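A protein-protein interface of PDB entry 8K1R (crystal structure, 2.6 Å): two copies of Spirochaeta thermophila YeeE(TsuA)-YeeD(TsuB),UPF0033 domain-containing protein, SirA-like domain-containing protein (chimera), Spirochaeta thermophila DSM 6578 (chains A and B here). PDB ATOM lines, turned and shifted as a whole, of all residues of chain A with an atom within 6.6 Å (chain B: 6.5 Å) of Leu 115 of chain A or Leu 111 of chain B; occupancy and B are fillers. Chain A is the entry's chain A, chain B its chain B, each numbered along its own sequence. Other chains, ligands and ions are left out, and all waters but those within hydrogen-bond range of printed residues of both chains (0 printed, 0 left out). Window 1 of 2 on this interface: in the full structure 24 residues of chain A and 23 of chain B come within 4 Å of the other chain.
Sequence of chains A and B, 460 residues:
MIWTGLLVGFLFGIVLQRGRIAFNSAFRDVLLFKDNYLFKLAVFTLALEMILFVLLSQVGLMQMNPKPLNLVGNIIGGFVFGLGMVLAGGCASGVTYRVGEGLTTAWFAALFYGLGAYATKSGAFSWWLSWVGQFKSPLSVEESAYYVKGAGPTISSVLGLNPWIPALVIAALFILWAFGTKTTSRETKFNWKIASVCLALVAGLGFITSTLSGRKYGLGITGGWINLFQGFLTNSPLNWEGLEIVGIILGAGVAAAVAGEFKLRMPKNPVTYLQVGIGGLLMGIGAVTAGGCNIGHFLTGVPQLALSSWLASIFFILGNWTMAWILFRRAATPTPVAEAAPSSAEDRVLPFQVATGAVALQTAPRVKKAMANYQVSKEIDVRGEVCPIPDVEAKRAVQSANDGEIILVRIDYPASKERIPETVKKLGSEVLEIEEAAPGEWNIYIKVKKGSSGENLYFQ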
ATOM      1  N   PHE A 108     -32.268  19.047  -5.931  1.00  0.00           N
ATOM      2  CA  PHE A 108     -32.571  18.751  -7.319  1.00  0.00           C
ATOM      3  C   PHE A 108     -31.790  19.669  -8.251  1.00  0.00           C
ATOM      4  O   PHE A 108     -31.162  19.208  -9.211  1.00  0.00           O
ATOM      5  CB  PHE A 108     -34.085  18.872  -7.546  1.00  0.00           C
ATOM      6  CG  PHE A 108     -34.641  17.823  -8.454  1.00  0.00           C
ATOM      7  CD1 PHE A 108     -34.582  16.482  -8.100  1.00  0.00           C
ATOM      8  CD2 PHE A 108     -35.195  18.167  -9.684  1.00  0.00           C
ATOM      9  CE1 PHE A 108     -35.083  15.489  -8.954  1.00  0.00           C
ATOM     10  CE2 PHE A 108     -35.706  17.188 -10.547  1.00  0.00           C
ATOM     11  CZ  PHE A 108     -35.639  15.848 -10.185  1.00  0.00           C
ATOM     12  N   ALA A 110     -29.072  21.383  -7.783  1.00  0.00           N
ATOM     13  CA  ALA A 110     -27.641  21.111  -7.733  1.00  0.00           C
ATOM     14  C   ALA A 110     -27.280  19.891  -8.569  1.00  0.00           C
ATOM     15  O   ALA A 110     -26.233  19.867  -9.235  1.00  0.00           O
ATOM     16  CB  ALA A 110     -27.205  20.901  -6.276  1.00  0.00           C
ATOM     17  N   LEU A 111     -28.116  18.846  -8.515  1.00  0.00           N
ATOM     18  CA  LEU A 111     -27.836  17.627  -9.265  1.00  0.00           C
ATOM     19  C   LEU A 111     -27.766  17.907 -10.759  1.00  0.00           C
ATOM     20  O   LEU A 111     -26.819  17.485 -11.443  1.00  0.00           O
ATOM     21  CB  LEU A 111     -28.906  16.579  -8.960  1.00  0.00           C
ATOM     22  CG  LEU A 111     -28.717  15.835  -7.636  1.00  0.00           C
ATOM     23  CD1 LEU A 111     -29.910  14.963  -7.345  1.00  0.00           C
ATOM     24  CD2 LEU A 111     -27.464  15.005  -7.741  1.00  0.00           C
ATOM     25  N   PHE A 112     -28.766  18.622 -11.287  1.00  0.00           N
ATOM     26  CA  PHE A 112     -28.764  18.942 -12.708  1.00  0.00           C
ATOM     27  C   PHE A 112     -27.721  20.000 -13.042  1.00  0.00           C
ATOM     28  O   PHE A 112     -27.196  20.022 -14.169  1.00  0.00           O
ATOM     29  CB  PHE A 112     -30.166  19.357 -13.147  1.00  0.00           C
ATOM     30  CG  PHE A 112     -31.125  18.202 -13.171  1.00  0.00           C
ATOM     31  CD1 PHE A 112     -31.225  17.389 -14.305  1.00  0.00           C
ATOM     32  CD2 PHE A 112     -31.887  17.880 -12.050  1.00  0.00           C
ATOM     33  CE1 PHE A 112     -32.080  16.288 -14.330  1.00  0.00           C
ATOM     34  CE2 PHE A 112     -32.750  16.783 -12.070  1.00  0.00           C
ATOM     35  CZ  PHE A 112     -32.842  15.982 -13.212  1.00  0.00           C
ATOM     36  N   TYR A 113     -27.383  20.858 -12.073  1.00  0.00           N
ATOM     37  CA  TYR A 113     -26.317  21.838 -12.279  1.00  0.00           C
ATOM     38  C   TYR A 113     -24.984  21.138 -12.464  1.00  0.00           C
ATOM     39  O   TYR A 113     -24.289  21.356 -13.468  1.00  0.00           O
ATOM     40  CB  TYR A 113     -26.258  22.804 -11.098  1.00  0.00           C
ATOM     41  CG  TYR A 113     -25.062  23.742 -11.068  1.00  0.00           C
ATOM     42  CD1 TYR A 113     -24.832  24.665 -12.091  1.00  0.00           C
ATOM     43  CD2 TYR A 113     -24.183  23.729  -9.986  1.00  0.00           C
ATOM     44  CE1 TYR A 113     -23.740  25.531 -12.044  1.00  0.00           C
ATOM     45  CE2 TYR A 113     -23.096  24.580  -9.925  1.00  0.00           C
ATOM     46  CZ  TYR A 113     -22.872  25.482 -10.947  1.00  0.00           C
ATOM     47  OH  TYR A 113     -21.777  26.323 -10.852  1.00  0.00           O
ATOM     48  N   GLY A 114     -24.631  20.264 -11.509  1.00  0.00           N
ATOM     49  CA  GLY A 114     -23.374  19.539 -11.594  1.00  0.00           C
ATOM     50  C   GLY A 114     -23.284  18.674 -12.831  1.00  0.00           C
ATOM     51  O   GLY A 114     -22.243  18.629 -13.490  1.00  0.00           O
ATOM     52  N   LEU A 115     -24.374  17.983 -13.173  1.00  0.00           N
ATOM     53  CA  LEU A 115     -24.338  17.086 -14.327  1.00  0.00           C
ATOM     54  C   LEU A 115     -24.249  17.877 -15.629  1.00  0.00           C
ATOM     55  O   LEU A 115     -23.453  17.541 -16.518  1.00  0.00           O
ATOM     56  CB  LEU A 115     -25.565  16.165 -14.317  1.00  0.00           C
ATOM     57  CG  LEU A 115     -25.731  15.151 -13.153  1.00  0.00           C
ATOM     58  CD1 LEU A 115     -27.136  14.522 -13.151  1.00  0.00           C
ATOM     59  CD2 LEU A 115     -24.658  14.048 -13.130  1.00  0.00           C
ATOM     60  N   GLY A 116     -25.035  18.955 -15.751  1.00  0.00           N
ATOM     61  CA  GLY A 116     -24.953  19.781 -16.948  1.00  0.00           C
ATOM     62  C   GLY A 116     -23.579  20.404 -17.155  1.00  0.00           C
ATOM     63  O   GLY A 116     -23.077  20.467 -18.286  1.00  0.00           O
ATOM     64  N   ALA A 117     -22.949  20.880 -16.064  1.00  0.00           N
ATOM     65  CA  ALA A 117     -21.609  21.453 -16.184  1.00  0.00           C
ATOM     66  C   ALA A 117     -20.583  20.396 -16.581  1.00  0.00           C
ATOM     67  O   ALA A 117     -19.711  20.659 -17.426  1.00  0.00           O
ATOM     68  CB  ALA A 117     -21.197  22.126 -14.878  1.00  0.00           C
ATOM     69  N   TYR A 118     -20.670  19.203 -15.966  1.00  0.00           N
ATOM     70  CA  TYR A 118     -19.786  18.087 -16.301  1.00  0.00           C
ATOM     71  C   TYR A 118     -19.960  17.685 -17.760  1.00  0.00           C
ATOM     72  O   TYR A 118     -18.974  17.478 -18.485  1.00  0.00           O
ATOM     73  CB  TYR A 118     -20.093  16.910 -15.367  1.00  0.00           C
ATOM     74  CG  TYR A 118     -19.073  15.778 -15.261  1.00  0.00           C
ATOM     75  CD1 TYR A 118     -18.422  15.271 -16.381  1.00  0.00           C
ATOM     76  CD2 TYR A 118     -18.834  15.155 -14.041  1.00  0.00           C
ATOM     77  CE1 TYR A 118     -17.519  14.227 -16.281  1.00  0.00           C
ATOM     78  CE2 TYR A 118     -17.938  14.093 -13.932  1.00  0.00           C
ATOM     79  CZ  TYR A 118     -17.285  13.640 -15.049  1.00  0.00           C
ATOM     80  OH  TYR A 118     -16.397  12.595 -14.939  1.00  0.00           O
ATOM     81  N   ALA A 119     -21.219  17.563 -18.205  1.00  0.00           N
ATOM     82  CA  ALA A 119     -21.509  17.208 -19.594  1.00  0.00           C
ATOM     83  C   ALA A 119     -21.048  18.281 -20.572  1.00  0.00           C
ATOM     84  O   ALA A 119     -20.733  17.981 -21.733  1.00  0.00           O
ATOM     85  CB  ALA A 119     -23.006  16.979 -19.766  1.00  0.00           C
ATOM     86  N   THR A 120     -21.041  19.543 -20.148  1.00  0.00           N
ATOM     87  CA  THR A 120     -20.541  20.595 -21.020  1.00  0.00           C
ATOM     88  C   THR A 120     -19.016  20.619 -21.048  1.00  0.00           C
ATOM     89  O   THR A 120     -18.423  20.935 -22.092  1.00  0.00           O
ATOM     90  CB  THR A 120     -21.107  21.945 -20.573  1.00  0.00           C
ATOM     91  OG1 THR A 120     -22.543  21.886 -20.576  1.00  0.00           O
ATOM     92  CG2 THR A 120     -20.633  23.075 -21.483  1.00  0.00           C
ATOM     93  N   PHE A 125     -22.210  17.700 -24.199  1.00  0.00           N
ATOM     94  CA  PHE A 125     -22.242  19.085 -24.670  1.00  0.00           C
ATOM     95  C   PHE A 125     -20.845  19.649 -24.936  1.00  0.00           C
ATOM     96  O   PHE A 125     -20.703  20.857 -25.133  1.00  0.00           O
ATOM     97  CB  PHE A 125     -22.979  19.971 -23.664  1.00  0.00           C
ATOM     98  CG  PHE A 125     -24.419  19.585 -23.436  1.00  0.00           C
ATOM     99  CD1 PHE A 125     -25.227  19.196 -24.487  1.00  0.00           C
ATOM    100  CD2 PHE A 125     -24.971  19.644 -22.163  1.00  0.00           C
ATOM    101  CE1 PHE A 125     -26.555  18.844 -24.271  1.00  0.00           C
ATOM    102  CE2 PHE A 125     -26.292  19.295 -21.934  1.00  0.00           C
ATOM    103  CZ  PHE A 125     -27.088  18.891 -22.995  1.00  0.00           C
ATOM    104  N   PHE A 229     -18.094  15.581  -8.609  1.00  0.00           N
ATOM    105  CA  PHE A 229     -18.649  14.543  -9.467  1.00  0.00           C
ATOM    106  C   PHE A 229     -17.553  13.659 -10.049  1.00  0.00           C
ATOM    107  O   PHE A 229     -17.713  12.434 -10.117  1.00  0.00           O
ATOM    108  CB  PHE A 229     -19.488  15.186 -10.581  1.00  0.00           C
ATOM    109  CG  PHE A 229     -20.930  15.421 -10.191  1.00  0.00           C
ATOM    110  CD1 PHE A 229     -21.898  14.439 -10.420  1.00  0.00           C
ATOM    111  CD2 PHE A 229     -21.314  16.604  -9.573  1.00  0.00           C
ATOM    112  CE1 PHE A 229     -23.224  14.642 -10.049  1.00  0.00           C
ATOM    113  CE2 PHE A 229     -22.631  16.812  -9.200  1.00  0.00           C
ATOM    114  CZ  PHE A 229     -23.588  15.828  -9.441  1.00  0.00           C
ATOM    115  N   LEU A 233     -17.367   9.648  -9.452  1.00  0.00           N
ATOM    116  CA  LEU A 233     -17.666   8.827 -10.617  1.00  0.00           C
ATOM    117  C   LEU A 233     -16.432   8.240 -11.297  1.00  0.00           C
ATOM    118  O   LEU A 233     -16.570   7.307 -12.099  1.00  0.00           O
ATOM    119  CB  LEU A 233     -18.482   9.636 -11.636  1.00  0.00           C
ATOM    120  CG  LEU A 233     -19.842  10.083 -11.106  1.00  0.00           C
ATOM    121  CD1 LEU A 233     -20.607  10.921 -12.116  1.00  0.00           C
ATOM    122  CD2 LEU A 233     -20.660   8.866 -10.667  1.00  0.00           C
ATOM    123  N   LEU A 281     -29.663  22.813 -15.193  1.00  0.00           N
ATOM    124  CA  LEU A 281     -29.020  22.427 -16.445  1.00  0.00           C
ATOM    125  C   LEU A 281     -28.557  23.646 -17.241  1.00  0.00           C
ATOM    126  O   LEU A 281     -27.448  23.667 -17.791  1.00  0.00           O
ATOM    127  CB  LEU A 281     -29.999  21.600 -17.280  1.00  0.00           C
ATOM    128  CG  LEU A 281     -29.983  20.085 -17.104  1.00  0.00           C
ATOM    129  CD1 LEU A 281     -31.154  19.439 -17.868  1.00  0.00           C
ATOM    130  CD2 LEU A 281     -28.628  19.527 -17.546  1.00  0.00           C
ATOM    131  N   GLY A 284     -25.473  24.890 -15.623  1.00  0.00           N
ATOM    132  CA  GLY A 284     -24.295  24.097 -15.929  1.00  0.00           C
ATOM    133  C   GLY A 284     -23.716  24.436 -17.286  1.00  0.00           C
ATOM    134  O   GLY A 284     -22.505  24.630 -17.432  1.00  0.00           O
ATOM    135  N   VAL B  95     -38.669   2.028  -9.991  1.00  0.00           N
ATOM    136  CA  VAL B  95     -38.228   3.420  -9.960  1.00  0.00           C
ATOM    137  C   VAL B  95     -38.231   3.992 -11.376  1.00  0.00           C
ATOM    138  O   VAL B  95     -38.809   5.057 -11.632  1.00  0.00           O
ATOM    139  CB  VAL B  95     -36.840   3.528  -9.294  1.00  0.00           C
ATOM    140  CG1 VAL B  95     -36.123   4.795  -9.723  1.00  0.00           C
ATOM    141  CG2 VAL B  95     -36.953   3.467  -7.755  1.00  0.00           C
ATOM    142  N   ALA B 106     -39.277   9.374  -7.577  1.00  0.00           N
ATOM    143  CA  ALA B 106     -38.598   8.421  -8.454  1.00  0.00           C
ATOM    144  C   ALA B 106     -37.513   9.096  -9.290  1.00  0.00           C
ATOM    145  O   ALA B 106     -36.501   8.460  -9.622  1.00  0.00           O
ATOM    146  CB  ALA B 106     -39.615   7.712  -9.339  1.00  0.00           C
ATOM    147  N   TRP B 107     -37.711  10.371  -9.647  1.00  0.00           N
ATOM    148  CA  TRP B 107     -36.639  11.153 -10.266  1.00  0.00           C
ATOM    149  C   TRP B 107     -35.428  11.200  -9.358  1.00  0.00           C
ATOM    150  O   TRP B 107     -34.288  10.972  -9.790  1.00  0.00           O
ATOM    151  CB  TRP B 107     -37.113  12.579 -10.560  1.00  0.00           C
ATOM    152  CG  TRP B 107     -38.321  12.654 -11.428  1.00  0.00           C
ATOM    153  CD1 TRP B 107     -38.988  11.605 -12.012  1.00  0.00           C
ATOM    154  CD2 TRP B 107     -39.010  13.841 -11.838  1.00  0.00           C
ATOM    155  NE1 TRP B 107     -40.050  12.068 -12.753  1.00  0.00           N
ATOM    156  CE2 TRP B 107     -40.084  13.437 -12.667  1.00  0.00           C
ATOM    157  CE3 TRP B 107     -38.818  15.206 -11.601  1.00  0.00           C
ATOM    158  CZ2 TRP B 107     -40.963  14.349 -13.246  1.00  0.00           C
ATOM    159  CZ3 TRP B 107     -39.698  16.109 -12.182  1.00  0.00           C
ATOM    160  CH2 TRP B 107     -40.760  15.673 -12.990  1.00  0.00           C
ATOM    161  N   PHE B 108     -35.673  11.483  -8.082  1.00  0.00           N
ATOM    162  CA  PHE B 108     -34.605  11.515  -7.098  1.00  0.00           C
ATOM    163  C   PHE B 108     -33.945  10.144  -6.956  1.00  0.00           C
ATOM    164  O   PHE B 108     -32.711  10.032  -6.986  1.00  0.00           O
ATOM    165  CB  PHE B 108     -35.169  12.018  -5.764  1.00  0.00           C
ATOM    166  CG  PHE B 108     -34.291  13.004  -5.090  1.00  0.00           C
ATOM    167  CD1 PHE B 108     -34.070  14.245  -5.659  1.00  0.00           C
ATOM    168  CD2 PHE B 108     -33.658  12.689  -3.895  1.00  0.00           C
ATOM    169  CE1 PHE B 108     -33.231  15.172  -5.052  1.00  0.00           C
ATOM    170  CE2 PHE B 108     -32.817  13.612  -3.270  1.00  0.00           C
ATOM    171  CZ  PHE B 108     -32.596  14.849  -3.855  1.00  0.00           C
ATOM    172  N   ALA B 109     -34.747   9.083  -6.815  1.00  0.00           N
ATOM    173  CA  ALA B 109     -34.170   7.756  -6.597  1.00  0.00           C
ATOM    174  C   ALA B 109     -33.359   7.285  -7.806  1.00  0.00           C
ATOM    175  O   ALA B 109     -32.317   6.634  -7.650  1.00  0.00           O
ATOM    176  CB  ALA B 109     -35.272   6.753  -6.262  1.00  0.00           C
ATOM    177  N   ALA B 110     -33.810   7.610  -9.020  1.00  0.00           N
ATOM    178  CA  ALA B 110     -33.083   7.167 -10.207  1.00  0.00           C
ATOM    179  C   ALA B 110     -31.745   7.884 -10.335  1.00  0.00           C
ATOM    180  O   ALA B 110     -30.746   7.280 -10.751  1.00  0.00           O
ATOM    181  CB  ALA B 110     -33.932   7.393 -11.462  1.00  0.00           C
ATOM    182  N   LEU B 111     -31.715   9.183 -10.001  1.00  0.00           N
ATOM    183  CA  LEU B 111     -30.466   9.935 -10.015  1.00  0.00           C
ATOM    184  C   LEU B 111     -29.420   9.289  -9.117  1.00  0.00           C
ATOM    185  O   LEU B 111     -28.312   8.968  -9.567  1.00  0.00           O
ATOM    186  CB  LEU B 111     -30.726  11.383  -9.590  1.00  0.00           C
ATOM    187  CG  LEU B 111     -31.216  12.256 -10.748  1.00  0.00           C
ATOM    188  CD1 LEU B 111     -32.028  13.461 -10.273  1.00  0.00           C
ATOM    189  CD2 LEU B 111     -30.016  12.690 -11.563  1.00  0.00           C
ATOM    190  N   PHE B 112     -29.750   9.083  -7.837  1.00  0.00           N
ATOM    191  CA  PHE B 112     -28.775   8.482  -6.930  1.00  0.00           C
ATOM    192  C   PHE B 112     -28.502   7.022  -7.284  1.00  0.00           C
ATOM    193  O   PHE B 112     -27.373   6.544  -7.088  1.00  0.00           O
ATOM    194  CB  PHE B 112     -29.235   8.647  -5.480  1.00  0.00           C
ATOM    195  CG  PHE B 112     -29.113  10.064  -4.992  1.00  0.00           C
ATOM    196  CD1 PHE B 112     -27.925  10.523  -4.439  1.00  0.00           C
ATOM    197  CD2 PHE B 112     -30.166  10.962  -5.134  1.00  0.00           C
ATOM    198  CE1 PHE B 112     -27.791  11.843  -4.016  1.00  0.00           C
ATOM    199  CE2 PHE B 112     -30.037  12.285  -4.708  1.00  0.00           C
ATOM    200  CZ  PHE B 112     -28.850  12.725  -4.151  1.00  0.00           C
ATOM    201  N   TYR B 113     -29.501   6.317  -7.838  1.00  0.00           N
ATOM    202  CA  TYR B 113     -29.286   4.953  -8.324  1.00  0.00           C
ATOM    203  C   TYR B 113     -28.235   4.932  -9.419  1.00  0.00           C
ATOM    204  O   TYR B 113     -27.248   4.189  -9.333  1.00  0.00           O
ATOM    205  CB  TYR B 113     -30.603   4.360  -8.835  1.00  0.00           C
ATOM    206  CG  TYR B 113     -30.493   3.010  -9.536  1.00  0.00           C
ATOM    207  CD1 TYR B 113     -29.941   1.899  -8.889  1.00  0.00           C
ATOM    208  CD2 TYR B 113     -30.977   2.839 -10.831  1.00  0.00           C
ATOM    209  CE1 TYR B 113     -29.852   0.661  -9.526  1.00  0.00           C
ATOM    210  CE2 TYR B 113     -30.891   1.612 -11.480  1.00  0.00           C
ATOM    211  CZ  TYR B 113     -30.332   0.527 -10.828  1.00  0.00           C
ATOM    212  OH  TYR B 113     -30.256  -0.686 -11.487  1.00  0.00           O
ATOM    213  N   GLY B 114     -28.428   5.761 -10.453  1.00  0.00           N
ATOM    214  CA  GLY B 114     -27.466   5.818 -11.537  1.00  0.00           C
ATOM    215  C   GLY B 114     -26.093   6.252 -11.065  1.00  0.00           C
ATOM    216  O   GLY B 114     -25.077   5.654 -11.433  1.00  0.00           O
ATOM    217  N   LEU B 115     -26.041   7.301 -10.247  1.00  0.00           N
ATOM    218  CA  LEU B 115     -24.743   7.795  -9.788  1.00  0.00           C
ATOM    219  C   LEU B 115     -24.044   6.761  -8.908  1.00  0.00           C
ATOM    220  O   LEU B 115     -22.856   6.477  -9.095  1.00  0.00           O
ATOM    221  CB  LEU B 115     -24.917   9.124  -9.052  1.00  0.00           C
ATOM    222  CG  LEU B 115     -25.463  10.331  -9.845  1.00  0.00           C
ATOM    223  CD1 LEU B 115     -25.862  11.434  -8.890  1.00  0.00           C
ATOM    224  CD2 LEU B 115     -24.494  10.886 -10.898  1.00  0.00           C
ATOM    225  N   GLY B 116     -24.780   6.149  -7.973  1.00  0.00           N
ATOM    226  CA  GLY B 116     -24.185   5.115  -7.134  1.00  0.00           C
ATOM    227  C   GLY B 116     -23.712   3.902  -7.918  1.00  0.00           C
ATOM    228  O   GLY B 116     -22.664   3.320  -7.612  1.00  0.00           O
ATOM    229  N   TRP B 225     -28.843   2.426 -17.230  1.00  0.00           N
ATOM    230  CA  TRP B 225     -28.645   3.707 -16.565  1.00  0.00           C
ATOM    231  C   TRP B 225     -27.185   4.129 -16.593  1.00  0.00           C
ATOM    232  O   TRP B 225     -26.887   5.322 -16.725  1.00  0.00           O
ATOM    233  CB  TRP B 225     -29.167   3.641 -15.142  1.00  0.00           C
ATOM    234  CG  TRP B 225     -30.624   3.941 -15.040  1.00  0.00           C
ATOM    235  CD1 TRP B 225     -31.626   3.056 -14.759  1.00  0.00           C
ATOM    236  CD2 TRP B 225     -31.252   5.221 -15.205  1.00  0.00           C
ATOM    237  NE1 TRP B 225     -32.845   3.709 -14.737  1.00  0.00           N
ATOM    238  CE2 TRP B 225     -32.643   5.034 -15.018  1.00  0.00           C
ATOM    239  CE3 TRP B 225     -30.778   6.500 -15.504  1.00  0.00           C
ATOM    240  CZ2 TRP B 225     -33.557   6.078 -15.108  1.00  0.00           C
ATOM    241  CZ3 TRP B 225     -31.690   7.539 -15.596  1.00  0.00           C
ATOM    242  CH2 TRP B 225     -33.063   7.324 -15.398  1.00  0.00           C
ATOM    243  N   PHE B 229     -25.687   7.612 -18.296  1.00  0.00           N
ATOM    244  CA  PHE B 229     -24.799   8.529 -17.587  1.00  0.00           C
ATOM    245  C   PHE B 229     -23.445   8.654 -18.289  1.00  0.00           C
ATOM    246  O   PHE B 229     -22.890   9.753 -18.375  1.00  0.00           O
ATOM    247  CB  PHE B 229     -24.626   8.070 -16.132  1.00  0.00           C
ATOM    248  CG  PHE B 229     -25.684   8.608 -15.203  1.00  0.00           C
ATOM    249  CD1 PHE B 229     -25.540   9.857 -14.610  1.00  0.00           C
ATOM    250  CD2 PHE B 229     -26.837   7.875 -14.941  1.00  0.00           C
ATOM    251  CE1 PHE B 229     -26.522  10.367 -13.754  1.00  0.00           C
ATOM    252  CE2 PHE B 229     -27.814   8.362 -14.096  1.00  0.00           C
ATOM    253  CZ  PHE B 229     -27.652   9.617 -13.493  1.00  0.00           C
ATOM    254  N   PHE B 232     -23.973  11.044 -21.410  1.00  0.00           N
ATOM    255  CA  PHE B 232     -24.103  12.455 -21.072  1.00  0.00           C
ATOM    256  C   PHE B 232     -22.790  13.037 -20.556  1.00  0.00           C
ATOM    257  O   PHE B 232     -22.423  14.170 -20.911  1.00  0.00           O
ATOM    258  CB  PHE B 232     -25.203  12.630 -20.023  1.00  0.00           C
ATOM    259  CG  PHE B 232     -25.719  14.045 -19.900  1.00  0.00           C
ATOM    260  CD1 PHE B 232     -26.127  14.747 -21.022  1.00  0.00           C
ATOM    261  CD2 PHE B 232     -25.807  14.659 -18.665  1.00  0.00           C
ATOM    262  CE1 PHE B 232     -26.610  16.036 -20.912  1.00  0.00           C
ATOM    263  CE2 PHE B 232     -26.295  15.942 -18.551  1.00  0.00           C
ATOM    264  CZ  PHE B 232     -26.703  16.630 -19.683  1.00  0.00           C
ATOM    265  N   LEU B 233     -22.070  12.280 -19.709  1.00  0.00           N
ATOM    266  CA  LEU B 233     -20.923  12.839 -19.003  1.00  0.00           C
ATOM    267  C   LEU B 233     -19.586  12.626 -19.719  1.00  0.00           C
ATOM    268  O   LEU B 233     -18.620  13.336 -19.414  1.00  0.00           O
ATOM    269  CB  LEU B 233     -20.855  12.263 -17.583  1.00  0.00           C
ATOM    270  CG  LEU B 233     -22.124  12.528 -16.764  1.00  0.00           C
ATOM    271  CD1 LEU B 233     -22.084  11.899 -15.337  1.00  0.00           C
ATOM    272  CD2 LEU B 233     -22.426  14.037 -16.716  1.00  0.00           C
ATOM    273  N   LEU B 281     -29.032   4.977  -3.826  1.00  0.00           N
ATOM    274  CA  LEU B 281     -27.601   4.717  -3.714  1.00  0.00           C
ATOM    275  C   LEU B 281     -27.328   3.276  -3.312  1.00  0.00           C
ATOM    276  O   LEU B 281     -26.421   2.631  -3.857  1.00  0.00           O
ATOM    277  CB  LEU B 281     -26.976   5.650  -2.682  1.00  0.00           C
ATOM    278  CG  LEU B 281     -26.653   7.092  -3.070  1.00  0.00           C
ATOM    279  CD1 LEU B 281     -26.273   7.908  -1.827  1.00  0.00           C
ATOM    280  CD2 LEU B 281     -25.559   7.141  -4.142  1.00  0.00           C
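The backbone carbonyl oxygen (O) of Ala 119 of chain A lies within hydrogen-bond range of the backbone NH (N) of Phe 125 of chain A, at 2.9 Å.
Among the printed residues, merely in contact across the chains: Phe 108 of chain A with Trp 107 of chain B, Phe 108 of chain A with Phe 108 of chain B, Phe 108 of chain A with Leu 111 of chain B, Leu 111 of chain A with Leu 111 of chain B, Leu 111 of chain A with Phe 112 of chain B, Phe 112 of chain A with Leu 111 of chain B, Leu 115 of chain A with Leu 111 of chain B, Leu 115 of chain A with Leu 115 of chain B, Leu 115 of chain A with Phe 232 of chain B, Leu 115 of chain A with Leu 233 of chain B, Tyr 118 of chain A with Leu 233 of chain B, Ala 119 of chain A with Phe 232 of chain B, Phe 125 of chain A with Phe 232 of chain B, Leu 233 of chain A with Leu 115 of chain B and Leu 233 of chain A with Leu 233 of chain B.
Of chain A, only Phe 108 (3.9 Å), Leu 111 (3.9 Å), Phe 112 (3.8 Å) and Leu 115 (3.8 Å) come within 4 Å of Leu 111 of chain B. Of the printed residues of chain A, Leu 115 of chain B touches Leu 115 and Leu 233. Of the printed residues of chain A, Leu 233 of chain B touches Leu 115, Tyr 118 and Leu 233. Of the printed residues of chain A, Trp 107 of chain B touches Phe 108. The nearest printed residue of chain A that does not touch Leu 111 of chain B is Phe 229 of chain A (7.2 Å).
Printed residues of chain A that touch a printed residue of chain B: Phe 108, Leu 111, Phe 112, Leu 115, Tyr 118, Ala 119, Phe 125 and Leu 233. Hydrophobic or aromatic side chains of chain B within 4 Å of the printed part of chain A: Trp 107, Phe 108, Leu 111, Phe 112, Leu 115, Phe 232 and Leu 233. Among the printed residues, 15 pairs touch across the chains.
Leu 111 of chain A touches Phe 112 of chain B, and with the chains exchanged Phe 112 of chain A touches Leu 111 of chain B. Leu 115 of chain A touches Leu 111 of chain B, but with the chains exchanged Leu 111 of chain A does not touch Leu 115 of chain B (4.1 Å). Leu 115 of chain B touches its own counterpart, Leu 115 of chain A. Leu 115 of chain A touches Leu 233 of chain B, and with the chains exchanged Leu 233 of chain A touches Leu 115 of chain B. 11 positions are printed for both chains. Of the 15 pairs that touch across the chains among the printed residues, 8 have their exchanged pair printed and touching as well.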
